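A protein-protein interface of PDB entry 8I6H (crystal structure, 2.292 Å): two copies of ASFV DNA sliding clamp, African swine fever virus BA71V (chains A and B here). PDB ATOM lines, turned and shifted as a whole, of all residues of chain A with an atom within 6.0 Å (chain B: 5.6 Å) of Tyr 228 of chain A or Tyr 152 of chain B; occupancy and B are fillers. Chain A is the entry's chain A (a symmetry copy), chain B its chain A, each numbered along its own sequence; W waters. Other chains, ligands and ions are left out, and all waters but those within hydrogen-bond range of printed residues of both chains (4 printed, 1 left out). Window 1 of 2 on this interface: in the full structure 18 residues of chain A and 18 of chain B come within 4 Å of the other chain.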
ATOM      1  N   THR A 194      -8.708   6.435 -14.627  1.00  0.00           N
ATOM      2  CA  THR A 194      -8.629   5.342 -13.678  1.00  0.00           C
ATOM      3  C   THR A 194      -7.547   4.341 -14.056  1.00  0.00           C
ATOM      4  O   THR A 194      -6.711   3.996 -13.228  1.00  0.00           O
ATOM      5  CB  THR A 194      -9.984   4.636 -13.570  1.00  0.00           C
ATOM      6  OG1 THR A 194     -10.877   5.464 -12.812  1.00  0.00           O
ATOM      7  CG2 THR A 194      -9.844   3.262 -12.925  1.00  0.00           C
ATOM      8  N   ASP A 197      -3.889   5.712 -14.243  1.00  0.00           N
ATOM      9  CA  ASP A 197      -3.450   5.839 -12.843  1.00  0.00           C
ATOM     10  C   ASP A 197      -3.063   4.486 -12.271  1.00  0.00           C
ATOM     11  O   ASP A 197      -2.068   4.358 -11.566  1.00  0.00           O
ATOM     12  CB  ASP A 197      -4.552   6.450 -11.968  1.00  0.00           C
ATOM     13  CG  ASP A 197      -4.573   7.972 -12.025  1.00  0.00           C
ATOM     14  OD1 ASP A 197      -4.016   8.556 -12.991  1.00  0.00           O
ATOM     15  OD2 ASP A 197      -5.170   8.581 -11.103  1.00  0.00           O
ATOM     16  N   LEU A 198      -3.867   3.470 -12.580  1.00  0.00           N
ATOM     17  CA  LEU A 198      -3.606   2.134 -12.072  1.00  0.00           C
ATOM     18  C   LEU A 198      -2.303   1.591 -12.662  1.00  0.00           C
ATOM     19  O   LEU A 198      -1.439   1.103 -11.926  1.00  0.00           O
ATOM     20  CB  LEU A 198      -4.782   1.192 -12.387  1.00  0.00           C
ATOM     21  CG  LEU A 198      -6.008   1.282 -11.462  1.00  0.00           C
ATOM     22  CD1 LEU A 198      -7.151   0.408 -11.991  1.00  0.00           C
ATOM     23  CD2 LEU A 198      -5.643   0.903 -10.037  1.00  0.00           C
ATOM     24  N   ASN A 200       0.312   2.973 -13.784  1.00  0.00           N
ATOM     25  CA  ASN A 200       1.517   3.561 -13.204  1.00  0.00           C
ATOM     26  C   ASN A 200       2.187   2.640 -12.190  1.00  0.00           C
ATOM     27  O   ASN A 200       3.401   2.676 -12.009  1.00  0.00           O
ATOM     28  CB  ASN A 200       1.193   4.880 -12.517  1.00  0.00           C
ATOM     29  CG  ASN A 200       0.906   5.992 -13.498  1.00  0.00           C
ATOM     30  OD1 ASN A 200       1.421   5.998 -14.609  1.00  0.00           O
ATOM     31  ND2 ASN A 200       0.087   6.952 -13.084  1.00  0.00           N
ATOM     32  N   TYR A 201       1.392   1.805 -11.530  1.00  0.00           N
ATOM     33  CA  TYR A 201       1.911   1.062 -10.395  1.00  0.00           C
ATOM     34  C   TYR A 201       1.557  -0.423 -10.399  1.00  0.00           C
ATOM     35  O   TYR A 201       2.151  -1.183  -9.653  1.00  0.00           O
ATOM     36  CB  TYR A 201       1.418   1.712  -9.086  1.00  0.00           C
ATOM     37  CG  TYR A 201       2.064   3.064  -8.744  1.00  0.00           C
ATOM     38  CD1 TYR A 201       3.382   3.135  -8.297  1.00  0.00           C
ATOM     39  CD2 TYR A 201       1.333   4.253  -8.814  1.00  0.00           C
ATOM     40  CE1 TYR A 201       3.966   4.358  -7.938  1.00  0.00           C
ATOM     41  CE2 TYR A 201       1.907   5.484  -8.459  1.00  0.00           C
ATOM     42  CZ  TYR A 201       3.228   5.528  -8.037  1.00  0.00           C
ATOM     43  OH  TYR A 201       3.823   6.742  -7.709  1.00  0.00           O
ATOM     44  N   LEU A 218     -11.994  -0.248  -6.312  1.00  0.00           N
ATOM     45  CA  LEU A 218     -10.887  -0.719  -7.136  1.00  0.00           C
ATOM     46  C   LEU A 218      -9.618  -0.548  -6.339  1.00  0.00           C
ATOM     47  O   LEU A 218      -9.345   0.553  -5.877  1.00  0.00           O
ATOM     48  CB  LEU A 218     -10.768   0.079  -8.433  1.00  0.00           C
ATOM     49  CG  LEU A 218     -12.060   0.346  -9.177  1.00  0.00           C
ATOM     50  CD1 LEU A 218     -11.753   1.214 -10.407  1.00  0.00           C
ATOM     51  CD2 LEU A 218     -12.660  -0.969  -9.596  1.00  0.00           C
ATOM     52  N   TYR A 219      -8.825  -1.597  -6.173  1.00  0.00           N
ATOM     53  CA  TYR A 219      -7.599  -1.423  -5.415  1.00  0.00           C
ATOM     54  C   TYR A 219      -6.565  -2.492  -5.676  1.00  0.00           C
ATOM     55  O   TYR A 219      -6.847  -3.523  -6.263  1.00  0.00           O
ATOM     56  CB  TYR A 219      -7.900  -1.370  -3.926  1.00  0.00           C
ATOM     57  CG  TYR A 219      -8.396  -2.680  -3.375  1.00  0.00           C
ATOM     58  CD1 TYR A 219      -7.524  -3.570  -2.764  1.00  0.00           C
ATOM     59  CD2 TYR A 219      -9.739  -3.037  -3.489  1.00  0.00           C
ATOM     60  CE1 TYR A 219      -7.982  -4.775  -2.264  1.00  0.00           C
ATOM     61  CE2 TYR A 219     -10.201  -4.237  -2.984  1.00  0.00           C
ATOM     62  CZ  TYR A 219      -9.319  -5.101  -2.374  1.00  0.00           C
ATOM     63  OH  TYR A 219      -9.769  -6.293  -1.874  1.00  0.00           O
ATOM     64  N   PHE A 220      -5.344  -2.220  -5.241  1.00  0.00           N
ATOM     65  CA  PHE A 220      -4.295  -3.212  -5.283  1.00  0.00           C
ATOM     66  C   PHE A 220      -3.414  -2.902  -4.105  1.00  0.00           C
ATOM     67  O   PHE A 220      -3.501  -1.807  -3.557  1.00  0.00           O
ATOM     68  CB  PHE A 220      -3.480  -3.148  -6.584  1.00  0.00           C
ATOM     69  CG  PHE A 220      -2.636  -1.906  -6.692  1.00  0.00           C
ATOM     70  CD1 PHE A 220      -1.409  -1.814  -6.035  1.00  0.00           C
ATOM     71  CD2 PHE A 220      -3.080  -0.823  -7.418  1.00  0.00           C
ATOM     72  CE1 PHE A 220      -0.643  -0.659  -6.117  1.00  0.00           C
ATOM     73  CE2 PHE A 220      -2.309   0.328  -7.512  1.00  0.00           C
ATOM     74  CZ  PHE A 220      -1.096   0.409  -6.850  1.00  0.00           C
ATOM     75  N   GLN A 221      -2.530  -3.837  -3.770  1.00  0.00           N
ATOM     76  CA  GLN A 221      -1.554  -3.649  -2.716  1.00  0.00           C
ATOM     77  C   GLN A 221      -0.182  -4.193  -3.111  1.00  0.00           C
ATOM     78  O   GLN A 221      -0.070  -5.351  -3.491  1.00  0.00           O
ATOM     79  CB  GLN A 221      -2.027  -4.325  -1.436  1.00  0.00           C
ATOM     80  CG  GLN A 221      -0.917  -4.470  -0.428  1.00  0.00           C
ATOM     81  CD  GLN A 221      -1.240  -5.434   0.710  1.00  0.00           C
ATOM     82  OE1 GLN A 221      -1.991  -6.403   0.538  1.00  0.00           O
ATOM     83  NE2 GLN A 221      -0.656  -5.176   1.875  1.00  0.00           N
ATOM     84  N   ILE A 226       3.812   0.736  -2.045  1.00  0.00           N
ATOM     85  CA  ILE A 226       2.620   1.536  -2.252  1.00  0.00           C
ATOM     86  C   ILE A 226       1.356   0.687  -2.372  1.00  0.00           C
ATOM     87  O   ILE A 226       1.379  -0.391  -2.952  1.00  0.00           O
ATOM     88  CB  ILE A 226       2.766   2.373  -3.524  1.00  0.00           C
ATOM     89  CG1 ILE A 226       1.470   3.118  -3.858  1.00  0.00           C
ATOM     90  CG2 ILE A 226       3.168   1.487  -4.677  1.00  0.00           C
ATOM     91  CD1 ILE A 226       1.489   3.789  -5.243  1.00  0.00           C
ATOM     92  N   SER A 227       0.261   1.192  -1.819  1.00  0.00           N
ATOM     93  CA  SER A 227      -1.055   0.637  -2.050  1.00  0.00           C
ATOM     94  C   SER A 227      -1.941   1.749  -2.529  1.00  0.00           C
ATOM     95  O   SER A 227      -1.713   2.918  -2.229  1.00  0.00           O
ATOM     96  CB  SER A 227      -1.635   0.005  -0.783  1.00  0.00           C
ATOM     97  OG  SER A 227      -0.819  -1.086  -0.431  1.00  0.00           O
ATOM     98  N   TYR A 228      -2.965   1.376  -3.268  1.00  0.00           N
ATOM     99  CA  TYR A 228      -3.843   2.349  -3.856  1.00  0.00           C
ATOM    100  C   TYR A 228      -5.245   1.819  -3.821  1.00  0.00           C
ATOM    101  O   TYR A 228      -5.482   0.619  -4.023  1.00  0.00           O
ATOM    102  CB  TYR A 228      -3.427   2.654  -5.295  1.00  0.00           C
ATOM    103  CG  TYR A 228      -4.363   3.583  -6.017  1.00  0.00           C
ATOM    104  CD1 TYR A 228      -4.386   4.950  -5.738  1.00  0.00           C
ATOM    105  CD2 TYR A 228      -5.230   3.094  -6.978  1.00  0.00           C
ATOM    106  CE1 TYR A 228      -5.252   5.800  -6.411  1.00  0.00           C
ATOM    107  CE2 TYR A 228      -6.094   3.933  -7.669  1.00  0.00           C
ATOM    108  CZ  TYR A 228      -6.099   5.285  -7.385  1.00  0.00           C
ATOM    109  OH  TYR A 228      -6.968   6.110  -8.073  1.00  0.00           O
ATOM    110  N   HIS A 229      -6.177   2.728  -3.598  1.00  0.00           N
ATOM    111  CA  HIS A 229      -7.548   2.354  -3.383  1.00  0.00           C
ATOM    112  C   HIS A 229      -8.438   3.395  -4.000  1.00  0.00           C
ATOM    113  O   HIS A 229      -8.370   4.567  -3.637  1.00  0.00           O
ATOM    114  CB  HIS A 229      -7.819   2.218  -1.882  1.00  0.00           C
ATOM    115  CG  HIS A 229      -9.223   1.833  -1.551  1.00  0.00           C
ATOM    116  ND1 HIS A 229      -9.908   2.388  -0.489  1.00  0.00           N
ATOM    117  CD2 HIS A 229     -10.052   0.930  -2.111  1.00  0.00           C
ATOM    118  CE1 HIS A 229     -11.109   1.842  -0.422  1.00  0.00           C
ATOM    119  NE2 HIS A 229     -11.228   0.959  -1.392  1.00  0.00           N
ATOM    120  N   GLU A 230      -9.279   2.968  -4.933  1.00  0.00           N
ATOM    121  CA  GLU A 230     -10.203   3.889  -5.563  1.00  0.00           C
ATOM    122  C   GLU A 230     -11.616   3.553  -5.130  1.00  0.00           C
ATOM    123  O   GLU A 230     -12.066   2.416  -5.281  1.00  0.00           O
ATOM    124  CB  GLU A 230     -10.080   3.824  -7.084  1.00  0.00           C
ATOM    125  CG  GLU A 230     -10.432   5.097  -7.783  1.00  0.00           C
ATOM    126  CD  GLU A 230      -9.997   5.099  -9.254  1.00  0.00           C
ATOM    127  OE1 GLU A 230     -10.874   4.909 -10.127  1.00  0.00           O
ATOM    128  OE2 GLU A 230      -8.781   5.277  -9.531  1.00  0.00           O
ATOM    129  N   MET B 114       2.473   9.160  -8.888  1.00  0.00           N
ATOM    130  CA  MET B 114       1.329   9.619  -8.092  1.00  0.00           C
ATOM    131  C   MET B 114       1.147  11.132  -8.166  1.00  0.00           C
ATOM    132  O   MET B 114       0.046  11.599  -8.474  1.00  0.00           O
ATOM    133  CB  MET B 114       1.465   9.198  -6.624  1.00  0.00           C
ATOM    134  CG  MET B 114       0.397   9.806  -5.716  1.00  0.00           C
ATOM    135  SD  MET B 114       0.704   9.522  -3.760  1.00  0.00           S
ATOM    136  CE  MET B 114       2.025  10.954  -3.367  1.00  0.00           C
ATOM    137  N   SER B 117      -0.052  12.217 -11.493  1.00  0.00           N
ATOM    138  CA  SER B 117      -1.426  11.863 -11.863  1.00  0.00           C
ATOM    139  C   SER B 117      -2.411  12.940 -11.406  1.00  0.00           C
ATOM    140  O   SER B 117      -3.570  12.913 -11.801  1.00  0.00           O
ATOM    141  CB  SER B 117      -1.831  10.495 -11.294  1.00  0.00           C
ATOM    142  OG  SER B 117      -2.209  10.595  -9.926  1.00  0.00           O
ATOM    143  N   LEU B 137       2.431   6.971   4.858  1.00  0.00           N
ATOM    144  CA  LEU B 137       1.885   8.290   4.627  1.00  0.00           C
ATOM    145  C   LEU B 137       0.717   8.182   3.672  1.00  0.00           C
ATOM    146  O   LEU B 137       0.856   7.653   2.567  1.00  0.00           O
ATOM    147  CB  LEU B 137       2.968   9.231   4.081  1.00  0.00           C
ATOM    148  CG  LEU B 137       2.678  10.730   4.093  1.00  0.00           C
ATOM    149  CD1 LEU B 137       2.444  11.226   5.565  1.00  0.00           C
ATOM    150  CD2 LEU B 137       3.844  11.486   3.441  1.00  0.00           C
ATOM    151  N   PHE B 138      -0.436   8.699   4.078  1.00  0.00           N
ATOM    152  CA  PHE B 138      -1.640   8.602   3.255  1.00  0.00           C
ATOM    153  C   PHE B 138      -1.801   9.848   2.416  1.00  0.00           C
ATOM    154  O   PHE B 138      -1.632  10.961   2.923  1.00  0.00           O
ATOM    155  CB  PHE B 138      -2.894   8.411   4.116  1.00  0.00           C
ATOM    156  CG  PHE B 138      -2.912   7.131   4.914  1.00  0.00           C
ATOM    157  CD1 PHE B 138      -2.193   7.025   6.088  1.00  0.00           C
ATOM    158  CD2 PHE B 138      -3.681   6.040   4.497  1.00  0.00           C
ATOM    159  CE1 PHE B 138      -2.217   5.863   6.833  1.00  0.00           C
ATOM    160  CE2 PHE B 138      -3.716   4.869   5.234  1.00  0.00           C
ATOM    161  CZ  PHE B 138      -2.982   4.778   6.407  1.00  0.00           C
ATOM    162  N   PHE B 139      -2.124   9.656   1.141  1.00  0.00           N
ATOM    163  CA  PHE B 139      -2.467  10.751   0.237  1.00  0.00           C
ATOM    164  C   PHE B 139      -3.845  10.478  -0.314  1.00  0.00           C
ATOM    165  O   PHE B 139      -4.057   9.446  -0.932  1.00  0.00           O
ATOM    166  CB  PHE B 139      -1.464  10.881  -0.916  1.00  0.00           C
ATOM    167  CG  PHE B 139      -0.095  11.276  -0.476  1.00  0.00           C
ATOM    168  CD1 PHE B 139       0.826  10.320  -0.093  1.00  0.00           C
ATOM    169  CD2 PHE B 139       0.268  12.618  -0.426  1.00  0.00           C
ATOM    170  CE1 PHE B 139       2.082  10.682   0.325  1.00  0.00           C
ATOM    171  CE2 PHE B 139       1.530  12.997  -0.011  1.00  0.00           C
ATOM    172  CZ  PHE B 139       2.441  12.033   0.362  1.00  0.00           C
ATOM    173  N   ILE B 140      -4.787  11.388  -0.080  1.00  0.00           N
ATOM    174  CA  ILE B 140      -6.153  11.185  -0.544  1.00  0.00           C
ATOM    175  C   ILE B 140      -6.565  12.309  -1.466  1.00  0.00           C
ATOM    176  O   ILE B 140      -6.494  13.471  -1.096  1.00  0.00           O
ATOM    177  CB  ILE B 140      -7.162  11.090   0.632  1.00  0.00           C
ATOM    178  CG1 ILE B 140      -6.782   9.951   1.569  1.00  0.00           C
ATOM    179  CG2 ILE B 140      -8.580  10.880   0.124  1.00  0.00           C
ATOM    180  CD1 ILE B 140      -6.119  10.433   2.859  1.00  0.00           C
ATOM    181  N   PHE B 141      -6.994  11.948  -2.670  1.00  0.00           N
ATOM    182  CA  PHE B 141      -7.464  12.921  -3.648  1.00  0.00           C
ATOM    183  C   PHE B 141      -8.936  12.716  -3.884  1.00  0.00           C
ATOM    184  O   PHE B 141      -9.373  11.589  -4.124  1.00  0.00           O
ATOM    185  CB  PHE B 141      -6.702  12.785  -4.962  1.00  0.00           C
ATOM    186  CG  PHE B 141      -5.228  12.937  -4.816  1.00  0.00           C
ATOM    187  CD1 PHE B 141      -4.633  14.191  -4.887  1.00  0.00           C
ATOM    188  CD2 PHE B 141      -4.424  11.831  -4.586  1.00  0.00           C
ATOM    189  CE1 PHE B 141      -3.260  14.337  -4.749  1.00  0.00           C
ATOM    190  CE2 PHE B 141      -3.037  11.975  -4.444  1.00  0.00           C
ATOM    191  CZ  PHE B 141      -2.461  13.232  -4.531  1.00  0.00           C
ATOM    192  N   LYS B 148     -15.730  10.347  -6.029  1.00  0.00           N
ATOM    193  CA  LYS B 148     -14.652   9.375  -6.099  1.00  0.00           C
ATOM    194  C   LYS B 148     -13.541   9.769  -5.151  1.00  0.00           C
ATOM    195  O   LYS B 148     -13.168  10.942  -5.067  1.00  0.00           O
ATOM    196  CB  LYS B 148     -14.101   9.241  -7.526  1.00  0.00           C
ATOM    197  CG  LYS B 148     -12.929   8.265  -7.602  1.00  0.00           C
ATOM    198  CD  LYS B 148     -12.405   8.048  -9.022  1.00  0.00           C
ATOM    199  CE  LYS B 148     -11.532   9.172  -9.505  1.00  0.00           C
ATOM    200  NZ  LYS B 148     -10.806   8.753 -10.755  1.00  0.00           N
ATOM    201  N   CYS B 150      -9.653   8.641  -4.022  1.00  0.00           N
ATOM    202  CA  CYS B 150      -8.464   7.872  -4.348  1.00  0.00           C
ATOM    203  C   CYS B 150      -7.471   7.987  -3.217  1.00  0.00           C
ATOM    204  O   CYS B 150      -7.009   9.089  -2.922  1.00  0.00           O
ATOM    205  CB  CYS B 150      -7.819   8.376  -5.638  1.00  0.00           C
ATOM    206  SG  CYS B 150      -8.942   8.401  -7.014  1.00  0.00           S
ATOM    207  N   THR B 151      -7.122   6.854  -2.616  1.00  0.00           N
ATOM    208  CA  THR B 151      -6.225   6.833  -1.479  1.00  0.00           C
ATOM    209  C   THR B 151      -4.922   6.090  -1.745  1.00  0.00           C
ATOM    210  O   THR B 151      -4.943   4.890  -2.004  1.00  0.00           O
ATOM    211  CB  THR B 151      -6.920   6.185  -0.254  1.00  0.00           C
ATOM    212  OG1 THR B 151      -8.118   6.906   0.043  1.00  0.00           O
ATOM    213  CG2 THR B 151      -5.990   6.187   0.936  1.00  0.00           C
ATOM    214  N   TYR B 152      -3.797   6.807  -1.640  1.00  0.00           N
ATOM    215  CA  TYR B 152      -2.473   6.207  -1.740  1.00  0.00           C
ATOM    216  C   TYR B 152      -1.931   5.926  -0.359  1.00  0.00           C
ATOM    217  O   TYR B 152      -2.062   6.747   0.537  1.00  0.00           O
ATOM    218  CB  TYR B 152      -1.493   7.129  -2.509  1.00  0.00           C
ATOM    219  CG  TYR B 152      -1.833   7.283  -3.977  1.00  0.00           C
ATOM    220  CD1 TYR B 152      -2.823   8.165  -4.394  1.00  0.00           C
ATOM    221  CD2 TYR B 152      -1.172   6.537  -4.934  1.00  0.00           C
ATOM    222  CE1 TYR B 152      -3.141   8.293  -5.722  1.00  0.00           C
ATOM    223  CE2 TYR B 152      -1.482   6.659  -6.272  1.00  0.00           C
ATOM    224  CZ  TYR B 152      -2.464   7.537  -6.663  1.00  0.00           C
ATOM    225  OH  TYR B 152      -2.766   7.635  -8.002  1.00  0.00           O
ATOM    226  N   GLN B 153      -1.321   4.765  -0.176  1.00  0.00           N
ATOM    227  CA  GLN B 153      -0.623   4.491   1.060  1.00  0.00           C
ATOM    228  C   GLN B 153       0.815   4.300   0.690  1.00  0.00           C
ATOM    229  O   GLN B 153       1.181   3.347   0.023  1.00  0.00           O
ATOM    230  CB  GLN B 153      -1.188   3.255   1.790  1.00  0.00           C
ATOM    231  CG  GLN B 153      -2.667   3.365   2.076  1.00  0.00           C
ATOM    232  CD  GLN B 153      -3.240   2.167   2.858  1.00  0.00           C
ATOM    233  OE1 GLN B 153      -2.645   1.686   3.826  1.00  0.00           O
ATOM    234  NE2 GLN B 153      -4.398   1.683   2.420  1.00  0.00           N
ATOM    235  N   ILE B 154       1.639   5.235   1.129  1.00  0.00           N
ATOM    236  CA  ILE B 154       3.014   5.279   0.708  1.00  0.00           C
ATOM    237  C   ILE B 154       3.925   4.876   1.847  1.00  0.00           C
ATOM    238  O   ILE B 154       3.830   5.413   2.946  1.00  0.00           O
ATOM    239  CB  ILE B 154       3.340   6.688   0.204  1.00  0.00           C
ATOM    240  CG1 ILE B 154       2.543   6.938  -1.077  1.00  0.00           C
ATOM    241  CG2 ILE B 154       4.839   6.860  -0.026  1.00  0.00           C
ATOM    242  CD1 ILE B 154       2.907   5.994  -2.176  1.00  0.00           C
HETATM  243  O   HOH W   1      -1.080   6.705 -10.163  1.00  0.00           O
HETATM  244  O   HOH W   2      -9.966   5.731  -1.216  1.00  0.00           O
HETATM  245  O   HOH W   3      -8.519   7.473 -11.018  1.00  0.00           O
HETATM  246  O   HOH W   4       1.007  10.034 -13.922  1.00  0.00           O
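No position is printed for both chains.
Among the printed residues, merely in contact across the chains: Thr 194 of chain A with Lys 148 of chain B (3.9 Å), Asp 197 of chain A with Ser 117 of chain B (3.4 Å), Ile 226 of chain A with Tyr 152 of chain B (3.8 Å), Ile 226 of chain A with Gln 153 of chain B (3.2 Å), Ile 226 of chain A with Ile 154 of chain B (3.6 Å), Ser 227 of chain A with Thr 151 of chain B (3.8 Å), Ser 227 of chain A with Tyr 152 of chain B (3.4 Å), Tyr 228 of chain A with Thr 151 of chain B (3.3 Å), Tyr 228 of chain A with Tyr 152 of chain B (3.3 Å), His 229 of chain A with Cys 150 of chain B (3.4 Å) and Glu 230 of chain A with Cys 150 of chain B (3.7 Å).
Of the 13 printed residues of chain B, 8 touch a printed residue of chain A. Printed residues of chain B that touch a printed residue of chain A: Met 114, Ser 117, Lys 148, Cys 150, Thr 151, Tyr 152, Gln 153 and Ile 154. Hydrophobic or aromatic side chains of chain A that line the printed part of chain B: Tyr 201, Ile 226, Tyr 228 and His 229. Among the printed residues, 16 pairs touch across the chains. Among the printed residues, Asp or Glu carboxylates within 4 Å of a Lys or Arg side-chain nitrogen of the other chain: Glu 230 of chain A with Lys 148 of chain B (3.9 Å).
Water W2 lies within hydrogen-bond range of the side-chain hydroxyl of Thr 151 of chain B (2.5 Å) and the backbone carbonyl oxygen of His 229 of chain A (3.1 Å). Water W3 bridges the side-chain amino group (NZ) of Lys 148 of chain B (2.6 Å) and the side-chain carboxylate (OE2) of Glu 230 of chain A (2.7 Å). Water W1 lies within hydrogen-bond range of OH of Tyr 152 of chain B, O of Asp 197 of chain A and ND2 of Asn 200 of chain A. Water W4 lies within hydrogen-bond range of ND2 of Asn 200 of chain A (3.3 Å) and N of Ser 117 of chain B (3.4 Å).
N of Met 114 of chain B lies within hydrogen-bond range of OH of Tyr 201 of chain A. NZ of Lys 148 of chain B is in salt-bridge range of OE1 of Glu 230 of chain A (3.9 Å). SG of Cys 150 of chain B lies within hydrogen-bond range of OH of Tyr 228 of chain A (3.2 Å). N of Thr 151 of chain B lies within hydrogen-bond range of O of His 229 of chain A (2.8 Å). The backbone NH (N) of Gln 153 of chain B sits at hydrogen-bond distance from the backbone carbonyl oxygen (O) of Ser 227 of chain A (2.8 Å).
N of Leu 137 of chain B is in hydrogen-bond range of O of Ile 154 of chain B, 2.8 Å away. The backbone carbonyl oxygen of Phe 139 of chain B sits at hydrogen-bond distance from the backbone NH of Tyr 152 of chain B (2.7 Å). N of Phe 141 of chain B sits at hydrogen-bond distance from O of Cys 150 of chain B, 2.9 Å away. The backbone carbonyl oxygen (O) of Leu 218 of chain A sits at hydrogen-bond distance from the backbone NH (N) of Glu 230 of chain A, 2.6 Å away. The backbone carbonyl oxygen (O) of Tyr 228 of chain A lies within hydrogen-bond range of the backbone NH (N) of Phe 220 of chain A, 3.1 Å away. The side-chain hydroxyl (OH) of Tyr 228 of chain A is in hydrogen-bond range of the side-chain carboxylate (OE2) of Glu 230 of chain A (2.5 Å).
Of the printed residues of chain B, Tyr 228 of chain A touches Cys 150 (3.2 Å), Thr 151 (3.3 Å) and Tyr 152 (3.3 Å). Of the printed residues of chain B, Ile 226 of chain A touches Tyr 152, Gln 153 and Ile 154. Printed residues of chain A within 4 Å of Met 114 of chain B: Tyr 201 (3.0 Å). Printed residues of chain B within 4 Å of Thr 194 of chain A: Lys 148. Printed residues of chain A within 4 Å of Ser 117 of chain B: Asp 197. The nearest residue of chain A that does not touch Tyr 152 of chain B is Asp 197 of chain A (4.04 Å).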
